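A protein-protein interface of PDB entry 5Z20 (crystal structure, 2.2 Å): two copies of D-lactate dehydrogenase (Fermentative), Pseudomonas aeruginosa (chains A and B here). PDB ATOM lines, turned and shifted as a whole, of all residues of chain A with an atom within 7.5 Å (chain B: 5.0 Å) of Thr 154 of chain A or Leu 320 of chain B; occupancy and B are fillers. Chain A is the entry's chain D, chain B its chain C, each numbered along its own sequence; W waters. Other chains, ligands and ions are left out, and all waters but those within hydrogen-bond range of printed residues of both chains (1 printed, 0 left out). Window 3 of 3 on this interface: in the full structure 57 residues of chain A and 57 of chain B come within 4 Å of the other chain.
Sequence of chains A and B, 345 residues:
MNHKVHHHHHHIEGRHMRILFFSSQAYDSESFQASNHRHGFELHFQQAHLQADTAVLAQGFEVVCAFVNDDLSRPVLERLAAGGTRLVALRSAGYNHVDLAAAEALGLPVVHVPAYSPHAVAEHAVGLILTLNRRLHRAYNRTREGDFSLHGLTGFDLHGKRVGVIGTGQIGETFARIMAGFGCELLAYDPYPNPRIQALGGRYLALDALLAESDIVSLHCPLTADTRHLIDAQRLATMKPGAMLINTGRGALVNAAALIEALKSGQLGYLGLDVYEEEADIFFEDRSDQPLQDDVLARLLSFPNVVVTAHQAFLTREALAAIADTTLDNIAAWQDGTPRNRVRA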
ATOM      1  N   LEU A 132      -1.637 -27.963 -32.037  1.00  0.00           N
ATOM      2  CA  LEU A 132      -2.609 -27.552 -33.048  1.00  0.00           C
ATOM      3  C   LEU A 132      -3.958 -27.246 -32.466  1.00  0.00           C
ATOM      4  O   LEU A 132      -4.566 -26.195 -32.760  1.00  0.00           O
ATOM      5  CB  LEU A 132      -2.757 -28.646 -34.081  1.00  0.00           C
ATOM      6  CG  LEU A 132      -1.565 -28.794 -35.016  1.00  0.00           C
ATOM      7  CD1 LEU A 132      -1.602 -30.169 -35.724  1.00  0.00           C
ATOM      8  CD2 LEU A 132      -1.613 -27.671 -36.052  1.00  0.00           C
ATOM      9  N   ASN A 133      -4.401 -28.083 -31.549  1.00  0.00           N
ATOM     10  CA  ASN A 133      -5.759 -27.948 -30.960  1.00  0.00           C
ATOM     11  C   ASN A 133      -5.875 -26.657 -30.174  1.00  0.00           C
ATOM     12  O   ASN A 133      -6.747 -25.824 -30.421  1.00  0.00           O
ATOM     13  CB  ASN A 133      -6.037 -29.170 -30.129  1.00  0.00           C
ATOM     14  CG  ASN A 133      -7.420 -29.177 -29.465  1.00  0.00           C
ATOM     15  OD1 ASN A 133      -8.021 -28.171 -29.207  1.00  0.00           O
ATOM     16  ND2 ASN A 133      -7.856 -30.367 -29.109  1.00  0.00           N
ATOM     17  N   ARG A 134      -4.951 -26.442 -29.266  1.00  0.00           N
ATOM     18  CA  ARG A 134      -5.006 -25.260 -28.388  1.00  0.00           C
ATOM     19  C   ARG A 134      -4.203 -24.058 -28.914  1.00  0.00           C
ATOM     20  O   ARG A 134      -4.059 -23.062 -28.224  1.00  0.00           O
ATOM     21  CB  ARG A 134      -4.548 -25.645 -26.999  1.00  0.00           C
ATOM     22  CG  ARG A 134      -5.211 -26.924 -26.424  1.00  0.00           C
ATOM     23  CD  ARG A 134      -6.747 -26.929 -26.429  1.00  0.00           C
ATOM     24  NE  ARG A 134      -7.233 -25.950 -25.482  1.00  0.00           N
ATOM     25  CZ  ARG A 134      -7.673 -26.221 -24.276  1.00  0.00           C
ATOM     26  NH1 ARG A 134      -7.767 -27.452 -23.869  1.00  0.00           N
ATOM     27  NH2 ARG A 134      -7.955 -25.214 -23.438  1.00  0.00           N
ATOM     28  N   ARG A 135      -3.685 -24.207 -30.125  1.00  0.00           N
ATOM     29  CA  ARG A 135      -2.921 -23.156 -30.758  1.00  0.00           C
ATOM     30  C   ARG A 135      -1.789 -22.662 -29.879  1.00  0.00           C
ATOM     31  O   ARG A 135      -1.551 -21.462 -29.765  1.00  0.00           O
ATOM     32  CB  ARG A 135      -3.842 -21.986 -31.108  1.00  0.00           C
ATOM     33  CG  ARG A 135      -4.749 -22.261 -32.293  1.00  0.00           C
ATOM     34  CD  ARG A 135      -6.075 -22.862 -31.855  1.00  0.00           C
ATOM     35  NE  ARG A 135      -7.100 -22.722 -32.887  1.00  0.00           N
ATOM     36  CZ  ARG A 135      -7.983 -23.662 -33.197  1.00  0.00           C
ATOM     37  NH1 ARG A 135      -7.972 -24.822 -32.552  1.00  0.00           N
ATOM     38  NH2 ARG A 135      -8.882 -23.446 -34.149  1.00  0.00           N
ATOM     39  N   LEU A 150      -7.126 -13.673 -26.913  1.00  0.00           N
ATOM     40  CA  LEU A 150      -7.429 -15.040 -27.167  1.00  0.00           C
ATOM     41  C   LEU A 150      -8.207 -15.338 -28.466  1.00  0.00           C
ATOM     42  O   LEU A 150      -8.446 -16.534 -28.752  1.00  0.00           O
ATOM     43  CB  LEU A 150      -8.177 -15.614 -25.992  1.00  0.00           C
ATOM     44  CG  LEU A 150      -7.471 -15.555 -24.662  1.00  0.00           C
ATOM     45  CD1 LEU A 150      -8.336 -16.234 -23.606  1.00  0.00           C
ATOM     46  CD2 LEU A 150      -6.093 -16.228 -24.701  1.00  0.00           C
ATOM     47  N   HIS A 151      -8.506 -14.333 -29.268  1.00  0.00           N
ATOM     48  CA  HIS A 151      -9.209 -14.609 -30.542  1.00  0.00           C
ATOM     49  C   HIS A 151      -8.421 -15.664 -31.367  1.00  0.00           C
ATOM     50  O   HIS A 151      -7.208 -15.641 -31.473  1.00  0.00           O
ATOM     51  CB  HIS A 151      -9.395 -13.335 -31.392  1.00  0.00           C
ATOM     52  CG  HIS A 151      -8.092 -12.763 -31.873  1.00  0.00           C
ATOM     53  ND1 HIS A 151      -7.449 -13.215 -33.009  1.00  0.00           N
ATOM     54  CD2 HIS A 151      -7.237 -11.885 -31.284  1.00  0.00           C
ATOM     55  CE1 HIS A 151      -6.318 -12.542 -33.176  1.00  0.00           C
ATOM     56  NE2 HIS A 151      -6.156 -11.739 -32.131  1.00  0.00           N
ATOM     57  N   GLY A 152      -9.151 -16.597 -31.937  1.00  0.00           N
ATOM     58  CA  GLY A 152      -8.619 -17.639 -32.821  1.00  0.00           C
ATOM     59  C   GLY A 152      -7.961 -18.784 -32.048  1.00  0.00           C
ATOM     60  O   GLY A 152      -7.518 -19.736 -32.656  1.00  0.00           O
ATOM     61  N   LEU A 153      -7.930 -18.746 -30.712  1.00  0.00           N
ATOM     62  CA  LEU A 153      -7.238 -19.823 -29.984  1.00  0.00           C
ATOM     63  C   LEU A 153      -8.156 -20.886 -29.384  1.00  0.00           C
ATOM     64  O   LEU A 153      -7.695 -21.792 -28.668  1.00  0.00           O
ATOM     65  CB  LEU A 153      -6.380 -19.230 -28.869  1.00  0.00           C
ATOM     66  CG  LEU A 153      -5.457 -18.077 -29.263  1.00  0.00           C
ATOM     67  CD1 LEU A 153      -4.556 -17.632 -28.092  1.00  0.00           C
ATOM     68  CD2 LEU A 153      -4.559 -18.501 -30.407  1.00  0.00           C
ATOM     69  N   THR A 154      -9.460 -20.778 -29.640  1.00  0.00           N
ATOM     70  CA  THR A 154     -10.434 -21.709 -29.054  1.00  0.00           C
ATOM     71  C   THR A 154     -10.201 -23.042 -29.628  1.00  0.00           C
ATOM     72  O   THR A 154     -10.163 -23.212 -30.822  1.00  0.00           O
ATOM     73  CB  THR A 154     -11.883 -21.262 -29.288  1.00  0.00           C
ATOM     74  OG1 THR A 154     -12.039 -20.028 -28.623  1.00  0.00           O
ATOM     75  CG2 THR A 154     -12.907 -22.250 -28.638  1.00  0.00           C
ATOM     76  N   GLY A 155      -9.999 -24.016 -28.765  1.00  0.00           N
ATOM     77  CA  GLY A 155      -9.756 -25.371 -29.275  1.00  0.00           C
ATOM     78  C   GLY A 155     -10.981 -26.245 -29.129  1.00  0.00           C
ATOM     79  O   GLY A 155     -12.112 -25.754 -29.069  1.00  0.00           O
ATOM     80  N   PHE A 156     -10.734 -27.542 -28.997  1.00  0.00           N
ATOM     81  CA  PHE A 156     -11.774 -28.550 -28.818  1.00  0.00           C
ATOM     82  C   PHE A 156     -11.347 -29.591 -27.795  1.00  0.00           C
ATOM     83  O   PHE A 156     -10.165 -29.902 -27.646  1.00  0.00           O
ATOM     84  CB  PHE A 156     -12.168 -29.181 -30.155  1.00  0.00           C
ATOM     85  CG  PHE A 156     -11.076 -29.938 -30.860  1.00  0.00           C
ATOM     86  CD1 PHE A 156     -10.927 -31.286 -30.650  1.00  0.00           C
ATOM     87  CD2 PHE A 156     -10.229 -29.307 -31.765  1.00  0.00           C
ATOM     88  CE1 PHE A 156      -9.931 -31.993 -31.321  1.00  0.00           C
ATOM     89  CE2 PHE A 156      -9.235 -30.009 -32.422  1.00  0.00           C
ATOM     90  CZ  PHE A 156      -9.130 -31.358 -32.244  1.00  0.00           C
ATOM     91  N   ASP A 157     -12.304 -30.133 -27.077  1.00  0.00           N
ATOM     92  CA  ASP A 157     -12.010 -31.194 -26.117  1.00  0.00           C
ATOM     93  C   ASP A 157     -11.640 -32.447 -26.903  1.00  0.00           C
ATOM     94  O   ASP A 157     -12.340 -32.823 -27.859  1.00  0.00           O
ATOM     95  CB  ASP A 157     -13.249 -31.509 -25.231  1.00  0.00           C
ATOM     96  CG  ASP A 157     -13.589 -30.361 -24.258  1.00  0.00           C
ATOM     97  OD1 ASP A 157     -12.872 -29.353 -24.238  1.00  0.00           O
ATOM     98  OD2 ASP A 157     -14.532 -30.534 -23.467  1.00  0.00           O
ATOM     99  N   TYR A 270      -6.617 -29.188 -39.707  1.00  0.00           N
ATOM    100  CA  TYR A 270      -5.294 -29.086 -39.050  1.00  0.00           C
ATOM    101  C   TYR A 270      -4.315 -30.086 -39.624  1.00  0.00           C
ATOM    102  O   TYR A 270      -4.712 -31.202 -40.000  1.00  0.00           O
ATOM    103  CB  TYR A 270      -5.409 -29.465 -37.570  1.00  0.00           C
ATOM    104  CG  TYR A 270      -6.472 -28.756 -36.769  1.00  0.00           C
ATOM    105  CD1 TYR A 270      -7.768 -29.215 -36.744  1.00  0.00           C
ATOM    106  CD2 TYR A 270      -6.159 -27.654 -35.987  1.00  0.00           C
ATOM    107  CE1 TYR A 270      -8.748 -28.596 -35.954  1.00  0.00           C
ATOM    108  CE2 TYR A 270      -7.126 -27.009 -35.237  1.00  0.00           C
ATOM    109  CZ  TYR A 270      -8.420 -27.511 -35.223  1.00  0.00           C
ATOM    110  OH  TYR A 270      -9.345 -26.888 -34.459  1.00  0.00           O
ATOM    111  N   TYR B  27     -15.665 -13.923 -27.733  1.00  0.00           N
ATOM    112  CA  TYR B  27     -16.049 -15.354 -27.589  1.00  0.00           C
ATOM    113  C   TYR B  27     -17.182 -15.459 -26.555  1.00  0.00           C
ATOM    114  O   TYR B  27     -17.921 -16.424 -26.537  1.00  0.00           O
ATOM    115  CB  TYR B  27     -14.811 -16.254 -27.207  1.00  0.00           C
ATOM    116  CG  TYR B  27     -13.931 -15.838 -25.988  1.00  0.00           C
ATOM    117  CD1 TYR B  27     -14.319 -16.152 -24.709  1.00  0.00           C
ATOM    118  CD2 TYR B  27     -12.702 -15.156 -26.141  1.00  0.00           C
ATOM    119  CE1 TYR B  27     -13.550 -15.762 -23.600  1.00  0.00           C
ATOM    120  CE2 TYR B  27     -11.933 -14.754 -25.042  1.00  0.00           C
ATOM    121  CZ  TYR B  27     -12.346 -15.088 -23.772  1.00  0.00           C
ATOM    122  OH  TYR B  27     -11.618 -14.714 -22.601  1.00  0.00           O
ATOM    123  N   SER B  31     -20.839 -16.932 -27.649  1.00  0.00           N
ATOM    124  CA  SER B  31     -21.348 -18.177 -27.085  1.00  0.00           C
ATOM    125  C   SER B  31     -22.665 -17.923 -26.333  1.00  0.00           C
ATOM    126  O   SER B  31     -23.597 -18.708 -26.421  1.00  0.00           O
ATOM    127  CB  SER B  31     -20.324 -18.885 -26.177  1.00  0.00           C
ATOM    128  OG  SER B  31     -19.907 -18.073 -25.095  1.00  0.00           O
ATOM    129  N   PHE B 314      -9.525 -23.028 -20.135  1.00  0.00           N
ATOM    130  CA  PHE B 314     -10.982 -23.252 -20.223  1.00  0.00           C
ATOM    131  C   PHE B 314     -11.472 -23.095 -21.640  1.00  0.00           C
ATOM    132  O   PHE B 314     -12.628 -23.378 -21.938  1.00  0.00           O
ATOM    133  CB  PHE B 314     -11.747 -22.225 -19.367  1.00  0.00           C
ATOM    134  CG  PHE B 314     -11.778 -20.845 -19.961  1.00  0.00           C
ATOM    135  CD1 PHE B 314     -10.728 -19.939 -19.790  1.00  0.00           C
ATOM    136  CD2 PHE B 314     -12.894 -20.411 -20.634  1.00  0.00           C
ATOM    137  CE1 PHE B 314     -10.765 -18.675 -20.378  1.00  0.00           C
ATOM    138  CE2 PHE B 314     -12.958 -19.129 -21.181  1.00  0.00           C
ATOM    139  CZ  PHE B 314     -11.881 -18.264 -21.080  1.00  0.00           C
ATOM    140  N   LEU B 315     -10.621 -22.668 -22.571  1.00  0.00           N
ATOM    141  CA  LEU B 315     -11.116 -22.163 -23.851  1.00  0.00           C
ATOM    142  C   LEU B 315     -11.190 -23.231 -24.939  1.00  0.00           C
ATOM    143  O   LEU B 315     -10.373 -23.246 -25.867  1.00  0.00           O
ATOM    144  CB  LEU B 315     -10.207 -20.977 -24.301  1.00  0.00           C
ATOM    145  CG  LEU B 315     -10.747 -20.118 -25.441  1.00  0.00           C
ATOM    146  CD1 LEU B 315     -11.735 -19.071 -24.924  1.00  0.00           C
ATOM    147  CD2 LEU B 315      -9.633 -19.404 -26.208  1.00  0.00           C
ATOM    148  N   THR B 316     -12.210 -24.069 -24.877  1.00  0.00           N
ATOM    149  CA  THR B 316     -12.589 -24.927 -25.974  1.00  0.00           C
ATOM    150  C   THR B 316     -14.106 -24.732 -26.353  1.00  0.00           C
ATOM    151  O   THR B 316     -14.855 -24.135 -25.561  1.00  0.00           O
ATOM    152  CB  THR B 316     -12.456 -26.404 -25.612  1.00  0.00           C
ATOM    153  OG1 THR B 316     -13.395 -26.723 -24.553  1.00  0.00           O
ATOM    154  CG2 THR B 316     -11.084 -26.674 -25.149  1.00  0.00           C
ATOM    155  N   ARG B 317     -14.501 -25.138 -27.564  1.00  0.00           N
ATOM    156  CA  ARG B 317     -15.876 -24.979 -28.021  1.00  0.00           C
ATOM    157  C   ARG B 317     -16.844 -25.559 -26.989  1.00  0.00           C
ATOM    158  O   ARG B 317     -17.839 -24.928 -26.677  1.00  0.00           O
ATOM    159  CB  ARG B 317     -16.157 -25.729 -29.319  1.00  0.00           C
ATOM    160  CG  ARG B 317     -15.339 -25.281 -30.482  1.00  0.00           C
ATOM    161  CD  ARG B 317     -16.002 -24.188 -31.276  1.00  0.00           C
ATOM    162  NE  ARG B 317     -15.005 -23.153 -31.548  1.00  0.00           N
ATOM    163  CZ  ARG B 317     -15.290 -21.895 -31.814  1.00  0.00           C
ATOM    164  NH1 ARG B 317     -16.555 -21.488 -31.879  1.00  0.00           N
ATOM    165  NH2 ARG B 317     -14.300 -21.041 -32.020  1.00  0.00           N
ATOM    166  N   GLU B 318     -16.536 -26.755 -26.486  1.00  0.00           N
ATOM    167  CA  GLU B 318     -17.462 -27.462 -25.641  1.00  0.00           C
ATOM    168  C   GLU B 318     -17.495 -26.800 -24.308  1.00  0.00           C
ATOM    169  O   GLU B 318     -18.557 -26.723 -23.711  1.00  0.00           O
ATOM    170  CB  GLU B 318     -17.074 -28.930 -25.484  1.00  0.00           C
ATOM    171  CG  GLU B 318     -17.136 -29.778 -26.795  1.00  0.00           C
ATOM    172  CD  GLU B 318     -15.883 -29.697 -27.676  1.00  0.00           C
ATOM    173  OE1 GLU B 318     -14.934 -28.951 -27.377  1.00  0.00           O
ATOM    174  OE2 GLU B 318     -15.846 -30.329 -28.746  1.00  0.00           O
ATOM    175  N   ALA B 319     -16.329 -26.348 -23.805  1.00  0.00           N
ATOM    176  CA  ALA B 319     -16.324 -25.655 -22.542  1.00  0.00           C
ATOM    177  C   ALA B 319     -17.204 -24.384 -22.613  1.00  0.00           C
ATOM    178  O   ALA B 319     -18.002 -24.098 -21.707  1.00  0.00           O
ATOM    179  CB  ALA B 319     -14.926 -25.309 -22.145  1.00  0.00           C
ATOM    180  N   LEU B 320     -17.029 -23.589 -23.652  1.00  0.00           N
ATOM    181  CA  LEU B 320     -17.742 -22.315 -23.763  1.00  0.00           C
ATOM    182  C   LEU B 320     -19.251 -22.537 -23.852  1.00  0.00           C
ATOM    183  O   LEU B 320     -20.011 -21.794 -23.235  1.00  0.00           O
ATOM    184  CB  LEU B 320     -17.269 -21.539 -24.999  1.00  0.00           C
ATOM    185  CG  LEU B 320     -15.836 -20.956 -24.860  1.00  0.00           C
ATOM    186  CD1 LEU B 320     -15.385 -20.390 -26.198  1.00  0.00           C
ATOM    187  CD2 LEU B 320     -15.841 -19.840 -23.848  1.00  0.00           C
ATOM    188  N   ALA B 321     -19.664 -23.558 -24.617  1.00  0.00           N
ATOM    189  CA  ALA B 321     -21.080 -23.819 -24.796  1.00  0.00           C
ATOM    190  C   ALA B 321     -21.670 -24.228 -23.463  1.00  0.00           C
ATOM    191  O   ALA B 321     -22.746 -23.759 -23.110  1.00  0.00           O
ATOM    192  CB  ALA B 321     -21.334 -24.912 -25.852  1.00  0.00           C
ATOM    193  N   ALA B 322     -20.935 -25.042 -22.695  1.00  0.00           N
ATOM    194  CA  ALA B 322     -21.457 -25.477 -21.422  1.00  0.00           C
ATOM    195  C   ALA B 322     -21.509 -24.311 -20.458  1.00  0.00           C
ATOM    196  O   ALA B 322     -22.412 -24.231 -19.620  1.00  0.00           O
ATOM    197  CB  ALA B 322     -20.633 -26.663 -20.846  1.00  0.00           C
ATOM    198  N   ILE B 323     -20.518 -23.441 -20.493  1.00  0.00           N
ATOM    199  CA  ILE B 323     -20.507 -22.320 -19.600  1.00  0.00           C
ATOM    200  C   ILE B 323     -21.756 -21.424 -19.865  1.00  0.00           C
ATOM    201  O   ILE B 323     -22.383 -20.932 -18.925  1.00  0.00           O
ATOM    202  CB  ILE B 323     -19.254 -21.490 -19.710  1.00  0.00           C
ATOM    203  CG1 ILE B 323     -18.094 -22.200 -19.026  1.00  0.00           C
ATOM    204  CG2 ILE B 323     -19.429 -20.095 -19.095  1.00  0.00           C
ATOM    205  CD1 ILE B 323     -16.775 -21.722 -19.546  1.00  0.00           C
ATOM    206  N   ALA B 324     -22.004 -21.125 -21.119  1.00  0.00           N
ATOM    207  CA  ALA B 324     -23.105 -20.263 -21.511  1.00  0.00           C
ATOM    208  C   ALA B 324     -24.446 -20.964 -21.153  1.00  0.00           C
ATOM    209  O   ALA B 324     -25.298 -20.343 -20.529  1.00  0.00           O
ATOM    210  CB  ALA B 324     -23.063 -19.940 -22.994  1.00  0.00           C
ATOM    211  N   ASP B 325     -24.617 -22.210 -21.538  1.00  0.00           N
ATOM    212  CA  ASP B 325     -25.865 -22.891 -21.223  1.00  0.00           C
ATOM    213  C   ASP B 325     -26.106 -22.990 -19.764  1.00  0.00           C
ATOM    214  O   ASP B 325     -27.250 -22.702 -19.295  1.00  0.00           O
ATOM    215  CB  ASP B 325     -25.894 -24.304 -21.760  1.00  0.00           C
ATOM    216  CG  ASP B 325     -25.892 -24.351 -23.265  1.00  0.00           C
ATOM    217  OD1 ASP B 325     -26.198 -23.322 -23.937  1.00  0.00           O
ATOM    218  OD2 ASP B 325     -25.522 -25.442 -23.811  1.00  0.00           O
HETATM  219  O   HOH W   1      -7.473 -23.003 -26.372  1.00  0.00           O
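O of Leu 315 of chain B is in hydrogen-bond range of N of Gly 155 of chain A (3.0 Å). OG1 of Thr 316 of chain B sits at hydrogen-bond distance from OD1 of Asp 157 of chain A. N of Arg 317 of chain B lies within hydrogen-bond range of O of Gly 155 of chain A. The side-chain carboxylate (OE1) of Glu 318 of chain B is in hydrogen-bond range of the backbone NH (N) of Asp 157 of chain A, at 2.9 Å.
OG of Ser 31 of chain B sits at hydrogen-bond distance from O of Tyr 27 of chain B, at 3.0 Å. The side-chain hydroxyl of Thr 316 of chain B lies within hydrogen-bond range of the backbone NH of Ala 319 of chain B (3.1 Å). The backbone carbonyl oxygen of Phe 156 of chain A is in hydrogen-bond range of the side-chain amide nitrogen of Asn 133 of chain A (2.8 Å). The guanidinium group (NH1) of Arg 135 of chain A lies within hydrogen-bond range of the backbone carbonyl oxygen (O) of Thr 154 of chain A, 3.2 Å away.
Among the printed residues, pairs that only touch across the chains: Gly 155 of chain A with Thr 316 of chain B (3.2 Å), Thr 154 of chain A with Leu 315 of chain B (3.4 Å), Thr 154 of chain A with Arg 317 of chain B (3.5 Å), Phe 156 of chain A with Glu 318 of chain B (3.5 Å), Arg 134 of chain A with Thr 316 of chain B (3.5 Å), Thr 154 of chain A with Thr 316 of chain B (3.6 Å), Leu 150 of chain A with Tyr 27 of chain B (3.8 Å), Arg 134 of chain A with Leu 315 of chain B (3.8 Å), Leu 153 of chain A with Leu 315 of chain B (3.8 Å), Phe 156 of chain A with Thr 316 of chain B (3.9 Å) and Thr 154 of chain A with Leu 320 of chain B (3.9 Å).
Of the printed residues of chain B, Arg 134 of chain A touches Leu 315 (3.8 Å) and Thr 316 (3.5 Å). Of chain B, only Leu 315, Thr 316, Arg 317 and Leu 320 come within 4 Å of Thr 154 of chain A. Of the printed residues of chain B, Gly 155 of chain A touches Leu 315, Thr 316 and Arg 317. Of the printed residues of chain B, Phe 156 of chain A touches Thr 316 (3.9 Å) and Glu 318 (3.5 Å). Phe 314 of chain B touches none of the printed residues of chain A. Of the printed residues of chain A, Thr 316 of chain B touches Arg 134, Thr 154, Gly 155, Phe 156 and Asp 157. Of the printed residues of chain A, Glu 318 of chain B touches Phe 156 (3.5 Å) and Asp 157 (2.9 Å). Leu 320 of chain B touches just one residue of chain A: Thr 154. Asp 325 of chain B touches none of the printed residues of chain A. The nearest residue of chain A that does not touch Leu 320 of chain B is Gly 155 of chain A (6.9 Å).
Of the 13 printed residues of chain A, 7 touch a printed residue of chain B. Printed residues of chain A that touch a printed residue of chain B: Arg 134, Leu 150, Leu 153, Thr 154, Gly 155, Phe 156 and Asp 157. Hydrophobic or aromatic side chains of chain A that line the printed part of chain B: Leu 150 and Phe 156. Of the 14 printed residues of chain B, 6 touch a printed residue of chain A. Hydrophobic or aromatic side chains of chain B that line the printed part of chain A: Tyr 27, Leu 315 and Leu 320. Among the printed residues, 15 pairs touch across the chains. Among the printed residues, no Asp or Glu carboxylate lies within 4 Å of a Lys or Arg side-chain nitrogen of the other chain.
No position is printed for both chains. Of the 15 pairs that touch across the chains among the printed residues, none has its exchanged pair printed and touching as well.
Water W1 lies within hydrogen-bond range of O of Leu 153 of chain A (2.6 Å), O of Leu 315 of chain B (3.0 Å) and NE of Arg 134 of chain A (3.1 Å).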
